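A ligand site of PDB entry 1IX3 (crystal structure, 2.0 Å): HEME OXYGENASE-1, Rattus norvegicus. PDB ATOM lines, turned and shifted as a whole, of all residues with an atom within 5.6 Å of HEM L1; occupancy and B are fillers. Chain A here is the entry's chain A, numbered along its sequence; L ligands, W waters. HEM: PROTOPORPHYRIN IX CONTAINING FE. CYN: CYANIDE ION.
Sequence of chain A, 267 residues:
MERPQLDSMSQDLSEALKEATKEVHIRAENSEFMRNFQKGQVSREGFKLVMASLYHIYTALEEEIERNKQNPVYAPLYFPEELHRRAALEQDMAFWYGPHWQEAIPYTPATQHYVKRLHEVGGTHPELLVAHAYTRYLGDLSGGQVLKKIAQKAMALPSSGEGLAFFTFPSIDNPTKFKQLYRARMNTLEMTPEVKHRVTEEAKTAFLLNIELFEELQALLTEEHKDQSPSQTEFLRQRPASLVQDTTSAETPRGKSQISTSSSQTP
The side-chain amino group (NZ) of Lys 179 lies within salt-bridge range of an oxygen (O2D) of HEM L1. The guanidinium group (NH2) of Arg 183 lies within salt-bridge range of an oxygen (O2D) of HEM L1, 2.6 Å away. An oxygen (O1D) of HEM L1 sits at hydrogen-bond distance from the side-chain hydroxyl of Tyr 134 (2.6 Å). N of Gly 144 sits at hydrogen-bond distance from N of CYN L2 (3.0 Å). A ring nitrogen (NE2) of His 25 binds an iron atom (FE) of HEM L1, at 2.2 Å.
O of Glu 29 is in hydrogen-bond range of NE2 of Gln 38 (2.8 Å). ND2 of Asn 210 sits at hydrogen-bond distance from OH of Tyr 114 (3.0 Å). The backbone carbonyl oxygen (O) of Gly 139 is in hydrogen-bond range of the backbone NH (N) of Gly 144 (2.8 Å). O of Gly 139 sits close to OG of Ser 142 (3.4 Å). The backbone carbonyl oxygen (O) of Leu 138 sits at hydrogen-bond distance from the side-chain hydroxyl (OG) of Ser 142 (2.7 Å). The guanidinium group (NH1) of Arg 136 lies within hydrogen-bond range of the side-chain amide oxygen (OD1) of Asn 210 (3.0 Å). The side-chain amide nitrogen (NE2) of Gln 38 lies close to the backbone carbonyl oxygen (O) of Met 34, 3.1 Å away. OE2 of Glu 29 is in hydrogen-bond range of ND1 of His 25 (2.8 Å).
Merely in contact with HEM L1: Ser 142 (3.2 Å), Arg 136 (3.3 Å), Thr 135 (3.3 Å), Leu 147 (3.3 Å), Glu 29 (3.3 Å), Gly 143 (3.4 Å), Gly 139 (3.4 Å), Met 34 (3.5 Å), Lys 18 (3.5 Å), Phe 207 (3.5 Å), Asn 210 (3.6 Å), Gln 38 (3.6 Å), Phe 214 (3.8 Å) and Leu 138 (3.9 Å). Hydrophobic or aromatic side chains within 4 Å of HEM L1: His 25, Met 34, Tyr 134, Leu 138, Leu 147, Phe 207 and Phe 214. The nearest printed residue that does not touch HEM L1 is Ala 28 (4.1 Å).
Water W1 lies within hydrogen-bond range of an oxygen (O1D) of HEM L1 (2.8 Å), the backbone carbonyl oxygen of Ser 14 (2.8 Å) and the guanidinium group of Arg 183 (3.0 Å). Water W2 lies within hydrogen-bond range of the side-chain hydroxyl of Thr 21 (2.9 Å) and the side-chain hydroxyl of Tyr 134 (3.4 Å).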
ATOM      1  N   SER A  14      -4.585 -11.108 -35.256  1.00  0.00           N
ATOM      2  CA  SER A  14      -5.233 -11.291 -33.956  1.00  0.00           C
ATOM      3  C   SER A  14      -4.323 -12.033 -32.972  1.00  0.00           C
ATOM      4  O   SER A  14      -4.314 -11.751 -31.777  1.00  0.00           O
ATOM      5  CB  SER A  14      -6.555 -12.035 -34.118  1.00  0.00           C
ATOM      6  OG  SER A  14      -6.351 -13.319 -34.670  1.00  0.00           O
ATOM      7  N   LEU A  17      -1.203  -9.674 -32.117  1.00  0.00           N
ATOM      8  CA  LEU A  17      -1.587  -8.655 -31.137  1.00  0.00           C
ATOM      9  C   LEU A  17      -1.726  -9.253 -29.737  1.00  0.00           C
ATOM     10  O   LEU A  17      -1.262  -8.674 -28.764  1.00  0.00           O
ATOM     11  CB  LEU A  17      -2.891  -7.976 -31.570  1.00  0.00           C
ATOM     12  CG  LEU A  17      -2.688  -6.869 -32.609  1.00  0.00           C
ATOM     13  CD1 LEU A  17      -4.008  -6.410 -33.172  1.00  0.00           C
ATOM     14  CD2 LEU A  17      -1.953  -5.690 -31.955  1.00  0.00           C
ATOM     15  N   LYS A  18      -2.359 -10.418 -29.651  1.00  0.00           N
ATOM     16  CA  LYS A  18      -2.523 -11.055 -28.349  1.00  0.00           C
ATOM     17  C   LYS A  18      -1.166 -11.383 -27.729  1.00  0.00           C
ATOM     18  O   LYS A  18      -0.937 -11.115 -26.540  1.00  0.00           O
ATOM     19  CB  LYS A  18      -3.361 -12.339 -28.497  1.00  0.00           C
ATOM     20  CG  LYS A  18      -3.635 -13.053 -27.186  1.00  0.00           C
ATOM     21  CD  LYS A  18      -4.752 -14.081 -27.324  1.00  0.00           C
ATOM     22  CE  LYS A  18      -4.407 -15.155 -28.338  1.00  0.00           C
ATOM     23  NZ  LYS A  18      -3.188 -15.923 -27.938  1.00  0.00           N
ATOM     24  N   THR A  21       0.828  -8.242 -26.600  1.00  0.00           N
ATOM     25  CA  THR A  21       0.309  -7.468 -25.467  1.00  0.00           C
ATOM     26  C   THR A  21       0.066  -8.276 -24.206  1.00  0.00           C
ATOM     27  O   THR A  21      -0.405  -7.752 -23.206  1.00  0.00           O
ATOM     28  CB  THR A  21      -1.015  -6.749 -25.840  1.00  0.00           C
ATOM     29  OG1 THR A  21      -1.991  -7.723 -26.253  1.00  0.00           O
ATOM     30  CG2 THR A  21      -0.773  -5.758 -26.977  1.00  0.00           C
ATOM     31  N   HIS A  25      -0.309  -6.541 -20.569  1.00  0.00           N
ATOM     32  CA  HIS A  25      -1.643  -6.738 -20.021  1.00  0.00           C
ATOM     33  C   HIS A  25      -1.537  -7.166 -18.552  1.00  0.00           C
ATOM     34  O   HIS A  25      -2.253  -6.657 -17.693  1.00  0.00           O
ATOM     35  CB  HIS A  25      -2.415  -7.807 -20.804  1.00  0.00           C
ATOM     36  CG  HIS A  25      -3.816  -8.020 -20.307  1.00  0.00           C
ATOM     37  ND1 HIS A  25      -4.090  -8.542 -19.051  1.00  0.00           N
ATOM     38  CD2 HIS A  25      -5.019  -7.737 -20.861  1.00  0.00           C
ATOM     39  CE1 HIS A  25      -5.395  -8.566 -18.867  1.00  0.00           C
ATOM     40  NE2 HIS A  25      -5.976  -8.076 -19.945  1.00  0.00           N
ATOM     41  N   ALA A  28      -0.732  -4.226 -16.543  1.00  0.00           N
ATOM     42  CA  ALA A  28      -1.872  -3.331 -16.403  1.00  0.00           C
ATOM     43  C   ALA A  28      -2.890  -3.827 -15.365  1.00  0.00           C
ATOM     44  O   ALA A  28      -3.370  -3.039 -14.544  1.00  0.00           O
ATOM     45  CB  ALA A  28      -2.568  -3.133 -17.758  1.00  0.00           C
ATOM     46  N   GLU A  29      -3.212  -5.111 -15.390  1.00  0.00           N
ATOM     47  CA  GLU A  29      -4.169  -5.644 -14.433  1.00  0.00           C
ATOM     48  C   GLU A  29      -3.603  -5.695 -13.014  1.00  0.00           C
ATOM     49  O   GLU A  29      -4.350  -5.903 -12.048  1.00  0.00           O
ATOM     50  CB  GLU A  29      -4.666  -7.030 -14.882  1.00  0.00           C
ATOM     51  CG  GLU A  29      -3.629  -8.120 -14.985  1.00  0.00           C
ATOM     52  CD  GLU A  29      -4.208  -9.382 -15.608  1.00  0.00           C
ATOM     53  OE1 GLU A  29      -5.214  -9.901 -15.079  1.00  0.00           O
ATOM     54  OE2 GLU A  29      -3.650  -9.869 -16.615  1.00  0.00           O
ATOM     55  N   MET A  34      -6.020  -0.899 -10.555  1.00  0.00           N
ATOM     56  CA  MET A  34      -6.725  -2.140 -10.879  1.00  0.00           C
ATOM     57  C   MET A  34      -6.700  -3.175  -9.765  1.00  0.00           C
ATOM     58  O   MET A  34      -7.633  -3.959  -9.621  1.00  0.00           O
ATOM     59  CB  MET A  34      -6.190  -2.743 -12.177  1.00  0.00           C
ATOM     60  CG  MET A  34      -6.625  -1.952 -13.410  1.00  0.00           C
ATOM     61  SD  MET A  34      -8.443  -1.823 -13.494  1.00  0.00           S
ATOM     62  CE  MET A  34      -8.675  -1.586 -15.254  1.00  0.00           C
ATOM     63  N   PHE A  37      -9.266  -1.915  -7.513  1.00  0.00           N
ATOM     64  CA  PHE A  37     -10.572  -2.154  -8.117  1.00  0.00           C
ATOM     65  C   PHE A  37     -10.999  -3.592  -7.887  1.00  0.00           C
ATOM     66  O   PHE A  37     -12.110  -3.857  -7.412  1.00  0.00           O
ATOM     67  CB  PHE A  37     -10.525  -1.830  -9.624  1.00  0.00           C
ATOM     68  CG  PHE A  37     -11.852  -2.006 -10.324  1.00  0.00           C
ATOM     69  CD1 PHE A  37     -12.221  -3.232 -10.850  1.00  0.00           C
ATOM     70  CD2 PHE A  37     -12.730  -0.932 -10.449  1.00  0.00           C
ATOM     71  CE1 PHE A  37     -13.446  -3.402 -11.477  1.00  0.00           C
ATOM     72  CE2 PHE A  37     -13.956  -1.092 -11.083  1.00  0.00           C
ATOM     73  CZ  PHE A  37     -14.319  -2.337 -11.600  1.00  0.00           C
ATOM     74  N   GLN A  38     -10.113  -4.537  -8.210  1.00  0.00           N
ATOM     75  CA  GLN A  38     -10.422  -5.957  -8.041  1.00  0.00           C
ATOM     76  C   GLN A  38     -10.612  -6.338  -6.571  1.00  0.00           C
ATOM     77  O   GLN A  38     -11.161  -7.399  -6.262  1.00  0.00           O
ATOM     78  CB  GLN A  38      -9.307  -6.813  -8.659  1.00  0.00           C
ATOM     79  CG  GLN A  38      -9.048  -6.491 -10.116  1.00  0.00           C
ATOM     80  CD  GLN A  38      -7.899  -7.308 -10.701  1.00  0.00           C
ATOM     81  OE1 GLN A  38      -8.030  -8.498 -10.951  1.00  0.00           O
ATOM     82  NE2 GLN A  38      -6.755  -6.649 -10.901  1.00  0.00           N
ATOM     83  N   TYR A 114      -4.061  10.651 -24.135  1.00  0.00           N
ATOM     84  CA  TYR A 114      -4.537   9.415 -24.755  1.00  0.00           C
ATOM     85  C   TYR A 114      -5.303   9.906 -25.988  1.00  0.00           C
ATOM     86  O   TYR A 114      -5.094   9.453 -27.116  1.00  0.00           O
ATOM     87  CB  TYR A 114      -5.480   8.681 -23.807  1.00  0.00           C
ATOM     88  CG  TYR A 114      -5.795   7.226 -24.139  1.00  0.00           C
ATOM     89  CD1 TYR A 114      -5.845   6.768 -25.460  1.00  0.00           C
ATOM     90  CD2 TYR A 114      -6.121   6.313 -23.116  1.00  0.00           C
ATOM     91  CE1 TYR A 114      -6.215   5.450 -25.753  1.00  0.00           C
ATOM     92  CE2 TYR A 114      -6.491   5.008 -23.403  1.00  0.00           C
ATOM     93  CZ  TYR A 114      -6.541   4.575 -24.725  1.00  0.00           C
ATOM     94  OH  TYR A 114      -6.953   3.291 -24.993  1.00  0.00           O
ATOM     95  N   TYR A 134      -8.504  -2.627 -30.949  1.00  0.00           N
ATOM     96  CA  TYR A 134      -8.244  -3.947 -30.377  1.00  0.00           C
ATOM     97  C   TYR A 134      -8.042  -3.820 -28.861  1.00  0.00           C
ATOM     98  O   TYR A 134      -8.715  -4.484 -28.070  1.00  0.00           O
ATOM     99  CB  TYR A 134      -6.993  -4.557 -31.005  1.00  0.00           C
ATOM    100  CG  TYR A 134      -6.385  -5.680 -30.179  1.00  0.00           C
ATOM    101  CD1 TYR A 134      -6.908  -6.975 -30.223  1.00  0.00           C
ATOM    102  CD2 TYR A 134      -5.307  -5.435 -29.327  1.00  0.00           C
ATOM    103  CE1 TYR A 134      -6.382  -7.998 -29.426  1.00  0.00           C
ATOM    104  CE2 TYR A 134      -4.764  -6.445 -28.524  1.00  0.00           C
ATOM    105  CZ  TYR A 134      -5.310  -7.720 -28.578  1.00  0.00           C
ATOM    106  OH  TYR A 134      -4.813  -8.714 -27.777  1.00  0.00           O
ATOM    107  N   THR A 135      -7.116  -2.946 -28.472  1.00  0.00           N
ATOM    108  CA  THR A 135      -6.795  -2.742 -27.070  1.00  0.00           C
ATOM    109  C   THR A 135      -8.000  -2.449 -26.200  1.00  0.00           C
ATOM    110  O   THR A 135      -8.146  -3.029 -25.120  1.00  0.00           O
ATOM    111  CB  THR A 135      -5.743  -1.623 -26.897  1.00  0.00           C
ATOM    112  OG1 THR A 135      -4.533  -1.995 -27.577  1.00  0.00           O
ATOM    113  CG2 THR A 135      -5.420  -1.411 -25.418  1.00  0.00           C
ATOM    114  N   ARG A 136      -8.878  -1.551 -26.654  1.00  0.00           N
ATOM    115  CA  ARG A 136     -10.057  -1.208 -25.864  1.00  0.00           C
ATOM    116  C   ARG A 136     -11.221  -2.185 -26.028  1.00  0.00           C
ATOM    117  O   ARG A 136     -11.617  -2.831 -25.052  1.00  0.00           O
ATOM    118  CB  ARG A 136     -10.517   0.212 -26.187  1.00  0.00           C
ATOM    119  CG  ARG A 136      -9.647   1.324 -25.581  1.00  0.00           C
ATOM    120  CD  ARG A 136      -9.418   1.137 -24.066  1.00  0.00           C
ATOM    121  NE  ARG A 136     -10.626   0.670 -23.384  1.00  0.00           N
ATOM    122  CZ  ARG A 136     -10.709   0.465 -22.069  1.00  0.00           C
ATOM    123  NH1 ARG A 136      -9.674   0.685 -21.282  1.00  0.00           N
ATOM    124  NH2 ARG A 136     -11.842  -0.011 -21.554  1.00  0.00           N
ATOM    125  N   LEU A 138     -11.739  -5.334 -27.554  1.00  0.00           N
ATOM    126  CA  LEU A 138     -11.603  -6.754 -27.249  1.00  0.00           C
ATOM    127  C   LEU A 138     -11.506  -7.000 -25.749  1.00  0.00           C
ATOM    128  O   LEU A 138     -11.881  -8.070 -25.271  1.00  0.00           O
ATOM    129  CB  LEU A 138     -10.411  -7.367 -27.986  1.00  0.00           C
ATOM    130  CG  LEU A 138     -10.595  -7.568 -29.497  1.00  0.00           C
ATOM    131  CD1 LEU A 138      -9.794  -8.796 -29.940  1.00  0.00           C
ATOM    132  CD2 LEU A 138     -12.067  -7.805 -29.830  1.00  0.00           C
ATOM    133  N   GLY A 139     -11.014  -6.003 -25.028  1.00  0.00           N
ATOM    134  CA  GLY A 139     -10.929  -6.114 -23.580  1.00  0.00           C
ATOM    135  C   GLY A 139     -12.335  -5.968 -23.027  1.00  0.00           C
ATOM    136  O   GLY A 139     -12.783  -6.763 -22.199  1.00  0.00           O
ATOM    137  N   SER A 142     -14.393  -8.994 -23.152  1.00  0.00           N
ATOM    138  CA  SER A 142     -13.969 -10.139 -22.351  1.00  0.00           C
ATOM    139  C   SER A 142     -13.710  -9.765 -20.898  1.00  0.00           C
ATOM    140  O   SER A 142     -14.609  -9.860 -20.058  1.00  0.00           O
ATOM    141  CB  SER A 142     -12.717 -10.786 -22.985  1.00  0.00           C
ATOM    142  OG  SER A 142     -11.696  -9.836 -23.221  1.00  0.00           O
ATOM    143  N   GLY A 143     -12.488  -9.340 -20.592  1.00  0.00           N
ATOM    144  CA  GLY A 143     -12.185  -8.967 -19.215  1.00  0.00           C
ATOM    145  C   GLY A 143     -13.121  -7.890 -18.683  1.00  0.00           C
ATOM    146  O   GLY A 143     -13.381  -7.814 -17.484  1.00  0.00           O
ATOM    147  N   GLY A 144     -13.624  -7.045 -19.581  1.00  0.00           N
ATOM    148  CA  GLY A 144     -14.532  -5.984 -19.174  1.00  0.00           C
ATOM    149  C   GLY A 144     -15.768  -6.557 -18.500  1.00  0.00           C
ATOM    150  O   GLY A 144     -16.397  -5.902 -17.676  1.00  0.00           O
ATOM    151  N   VAL A 146     -15.724  -9.059 -16.488  1.00  0.00           N
ATOM    152  CA  VAL A 146     -15.328  -9.360 -15.116  1.00  0.00           C
ATOM    153  C   VAL A 146     -15.333  -8.047 -14.325  1.00  0.00           C
ATOM    154  O   VAL A 146     -15.747  -8.000 -13.172  1.00  0.00           O
ATOM    155  CB  VAL A 146     -13.908  -9.976 -15.072  1.00  0.00           C
ATOM    156  CG1 VAL A 146     -13.469 -10.191 -13.634  1.00  0.00           C
ATOM    157  CG2 VAL A 146     -13.887 -11.299 -15.827  1.00  0.00           C
ATOM    158  N   LEU A 147     -14.854  -6.978 -14.956  1.00  0.00           N
ATOM    159  CA  LEU A 147     -14.825  -5.666 -14.319  1.00  0.00           C
ATOM    160  C   LEU A 147     -16.239  -5.247 -13.968  1.00  0.00           C
ATOM    161  O   LEU A 147     -16.494  -4.672 -12.913  1.00  0.00           O
ATOM    162  CB  LEU A 147     -14.197  -4.627 -15.248  1.00  0.00           C
ATOM    163  CG  LEU A 147     -12.748  -4.879 -15.679  1.00  0.00           C
ATOM    164  CD1 LEU A 147     -12.199  -3.655 -16.395  1.00  0.00           C
ATOM    165  CD2 LEU A 147     -11.919  -5.203 -14.461  1.00  0.00           C
ATOM    166  N   ILE A 150     -17.388  -6.983 -10.874  1.00  0.00           N
ATOM    167  CA  ILE A 150     -16.734  -6.399  -9.711  1.00  0.00           C
ATOM    168  C   ILE A 150     -17.441  -5.108  -9.325  1.00  0.00           C
ATOM    169  O   ILE A 150     -17.766  -4.895  -8.151  1.00  0.00           O
ATOM    170  CB  ILE A 150     -15.243  -6.115  -9.996  1.00  0.00           C
ATOM    171  CG1 ILE A 150     -14.510  -7.439 -10.266  1.00  0.00           C
ATOM    172  CG2 ILE A 150     -14.613  -5.399  -8.814  1.00  0.00           C
ATOM    173  CD1 ILE A 150     -13.065  -7.260 -10.674  1.00  0.00           C
ATOM    174  N   LYS A 179     -16.430 -11.300 -30.310  1.00  0.00           N
ATOM    175  CA  LYS A 179     -14.984 -11.129 -30.243  1.00  0.00           C
ATOM    176  C   LYS A 179     -14.294 -12.041 -31.248  1.00  0.00           C
ATOM    177  O   LYS A 179     -13.306 -11.667 -31.882  1.00  0.00           O
ATOM    178  CB  LYS A 179     -14.479 -11.434 -28.825  1.00  0.00           C
ATOM    179  CG  LYS A 179     -12.971 -11.373 -28.678  1.00  0.00           C
ATOM    180  CD  LYS A 179     -12.560 -11.657 -27.243  1.00  0.00           C
ATOM    181  CE  LYS A 179     -11.050 -11.756 -27.108  1.00  0.00           C
ATOM    182  NZ  LYS A 179     -10.642 -12.146 -25.730  1.00  0.00           N
ATOM    183  N   ARG A 183     -12.007 -10.808 -34.365  1.00  0.00           N
ATOM    184  CA  ARG A 183     -10.660 -11.350 -34.569  1.00  0.00           C
ATOM    185  C   ARG A 183     -10.480 -11.814 -36.009  1.00  0.00           C
ATOM    186  O   ARG A 183      -9.463 -11.530 -36.637  1.00  0.00           O
ATOM    187  CB  ARG A 183     -10.425 -12.547 -33.644  1.00  0.00           C
ATOM    188  CG  ARG A 183      -9.978 -12.204 -32.246  1.00  0.00           C
ATOM    189  CD  ARG A 183     -10.070 -13.456 -31.386  1.00  0.00           C
ATOM    190  NE  ARG A 183      -9.304 -13.366 -30.146  1.00  0.00           N
ATOM    191  CZ  ARG A 183      -9.344 -14.301 -29.190  1.00  0.00           C
ATOM    192  NH1 ARG A 183     -10.120 -15.367 -29.342  1.00  0.00           N
ATOM    193  NH2 ARG A 183      -8.608 -14.170 -28.095  1.00  0.00           N
ATOM    194  N   PHE A 207      -1.776   0.258 -24.482  1.00  0.00           N
ATOM    195  CA  PHE A 207      -1.844  -0.318 -23.137  1.00  0.00           C
ATOM    196  C   PHE A 207      -1.188   0.625 -22.124  1.00  0.00           C
ATOM    197  O   PHE A 207      -1.729   0.871 -21.044  1.00  0.00           O
ATOM    198  CB  PHE A 207      -1.139  -1.671 -23.080  1.00  0.00           C
ATOM    199  CG  PHE A 207      -2.064  -2.845 -23.230  1.00  0.00           C
ATOM    200  CD1 PHE A 207      -2.433  -3.307 -24.498  1.00  0.00           C
ATOM    201  CD2 PHE A 207      -2.575  -3.488 -22.110  1.00  0.00           C
ATOM    202  CE1 PHE A 207      -3.308  -4.382 -24.639  1.00  0.00           C
ATOM    203  CE2 PHE A 207      -3.456  -4.578 -22.236  1.00  0.00           C
ATOM    204  CZ  PHE A 207      -3.825  -5.015 -23.504  1.00  0.00           C
ATOM    205  N   ASN A 210      -3.191   3.518 -21.122  1.00  0.00           N
ATOM    206  CA  ASN A 210      -4.218   3.119 -20.168  1.00  0.00           C
ATOM    207  C   ASN A 210      -3.629   3.022 -18.767  1.00  0.00           C
ATOM    208  O   ASN A 210      -4.238   3.470 -17.795  1.00  0.00           O
ATOM    209  CB  ASN A 210      -4.833   1.787 -20.590  1.00  0.00           C
ATOM    210  CG  ASN A 210      -5.890   1.946 -21.663  1.00  0.00           C
ATOM    211  OD1 ASN A 210      -7.052   2.234 -21.366  1.00  0.00           O
ATOM    212  ND2 ASN A 210      -5.482   1.786 -22.922  1.00  0.00           N
ATOM    213  N   PHE A 214      -4.864   5.063 -15.426  1.00  0.00           N
ATOM    214  CA  PHE A 214      -5.223   4.430 -14.173  1.00  0.00           C
ATOM    215  C   PHE A 214      -4.318   4.775 -13.008  1.00  0.00           C
ATOM    216  O   PHE A 214      -4.779   4.899 -11.869  1.00  0.00           O
ATOM    217  CB  PHE A 214      -5.300   2.912 -14.366  1.00  0.00           C
ATOM    218  CG  PHE A 214      -6.433   2.476 -15.264  1.00  0.00           C
ATOM    219  CD1 PHE A 214      -7.734   2.907 -15.008  1.00  0.00           C
ATOM    220  CD2 PHE A 214      -6.198   1.650 -16.353  1.00  0.00           C
ATOM    221  CE1 PHE A 214      -8.782   2.512 -15.842  1.00  0.00           C
ATOM    222  CE2 PHE A 214      -7.240   1.258 -17.194  1.00  0.00           C
ATOM    223  CZ  PHE A 214      -8.536   1.694 -16.932  1.00  0.00           C
HETATM  224  CHA HEM L   1      -8.640  -9.881 -22.349  1.00  0.00           C
HETATM  225  CHB HEM L   1      -8.897  -9.565 -17.521  1.00  0.00           C
HETATM  226  CHC HEM L   1      -7.357  -4.990 -17.743  1.00  0.00           C
HETATM  227  CHD HEM L   1      -7.275  -5.221 -22.560  1.00  0.00           C
HETATM  228  C1A HEM L   1      -8.907 -10.205 -20.998  1.00  0.00           C
HETATM  229  C2A HEM L   1      -9.442 -11.464 -20.528  1.00  0.00           C
HETATM  230  C3A HEM L   1      -9.511 -11.385 -19.167  1.00  0.00           C
HETATM  231  C4A HEM L   1      -9.016 -10.059 -18.821  1.00  0.00           C
HETATM  232  CMA HEM L   1     -10.008 -12.424 -18.184  1.00  0.00           C
HETATM  233  CAA HEM L   1      -9.852 -12.639 -21.413  1.00  0.00           C
HETATM  234  CBA HEM L   1      -8.736 -13.695 -21.629  1.00  0.00           C
HETATM  235  CGA HEM L   1      -9.150 -14.920 -22.205  1.00  0.00           C
HETATM  236  O1A HEM L   1      -8.858 -15.064 -23.455  1.00  0.00           O
HETATM  237  O2A HEM L   1      -9.745 -15.827 -21.589  1.00  0.00           O
HETATM  238  C1B HEM L   1      -8.621  -8.248 -17.167  1.00  0.00           C
HETATM  239  C2B HEM L   1      -8.747  -7.728 -15.807  1.00  0.00           C
HETATM  240  C3B HEM L   1      -8.117  -6.497 -15.833  1.00  0.00           C
HETATM  241  C4B HEM L   1      -7.864  -6.203 -17.253  1.00  0.00           C
HETATM  242  CMB HEM L   1      -9.437  -8.472 -14.651  1.00  0.00           C
HETATM  243  CAB HEM L   1      -7.668  -5.592 -14.675  1.00  0.00           C
HETATM  244  CBB HEM L   1      -8.713  -5.263 -13.583  1.00  0.00           C
HETATM  245  C1C HEM L   1      -7.178  -4.652 -19.062  1.00  0.00           C
HETATM  246  C2C HEM L   1      -6.730  -3.332 -19.532  1.00  0.00           C
HETATM  247  C3C HEM L   1      -6.666  -3.440 -20.884  1.00  0.00           C
HETATM  248  C4C HEM L   1      -7.121  -4.762 -21.250  1.00  0.00           C
HETATM  249  CMC HEM L   1      -6.431  -2.149 -18.623  1.00  0.00           C
HETATM  250  CAC HEM L   1      -6.170  -2.364 -21.876  1.00  0.00           C
HETATM  251  CBC HEM L   1      -7.256  -1.296 -22.191  1.00  0.00           C
HETATM  252  C1D HEM L   1      -7.578  -6.536 -22.950  1.00  0.00           C
HETATM  253  C2D HEM L   1      -7.561  -7.026 -24.345  1.00  0.00           C
HETATM  254  C3D HEM L   1      -7.967  -8.302 -24.280  1.00  0.00           C
HETATM  255  C4D HEM L   1      -8.196  -8.628 -22.843  1.00  0.00           C
HETATM  256  CMD HEM L   1      -7.165  -6.177 -25.539  1.00  0.00           C
HETATM  257  CAD HEM L   1      -8.203  -9.309 -25.396  1.00  0.00           C
HETATM  258  CBD HEM L   1      -7.008 -10.341 -25.561  1.00  0.00           C
HETATM  259  CGD HEM L   1      -7.123 -11.106 -26.744  1.00  0.00           C
HETATM  260  O1D HEM L   1      -6.399 -10.818 -27.744  1.00  0.00           O
HETATM  261  O2D HEM L   1      -7.926 -12.062 -26.819  1.00  0.00           O
HETATM  262  NA  HEM L   1      -8.679  -9.333 -19.959  1.00  0.00           N
HETATM  263  NB  HEM L   1      -8.179  -7.278 -18.063  1.00  0.00           N
HETATM  264  NC  HEM L   1      -7.410  -5.518 -20.144  1.00  0.00           N
HETATM  265  ND  HEM L   1      -7.927  -7.551 -22.057  1.00  0.00           N
HETATM  266 FE   HEM L   1      -8.041  -7.424 -20.062  1.00  0.00          FE
HETATM  267  C   CYN L   2      -9.944  -6.635 -20.225  1.00  0.00           C
HETATM  268  N   CYN L   2     -10.848  -6.020 -20.159  1.00  0.00           N
HETATM  269  O   HOH W   1      -6.742 -11.735 -30.350  1.00  0.00           O
HETATM  270  O   HOH W   2      -4.246  -8.124 -24.519  1.00  0.00           O
HETATM  271  O   HOH W   3     -10.037  -2.865 -22.884  1.00  0.00           O
HETATM  272  O   HOH W   4      -6.826 -13.864 -24.807  1.00  0.00           O
HETATM  273  O   HOH W   5      -6.617 -11.822 -16.469  1.00  0.00           O
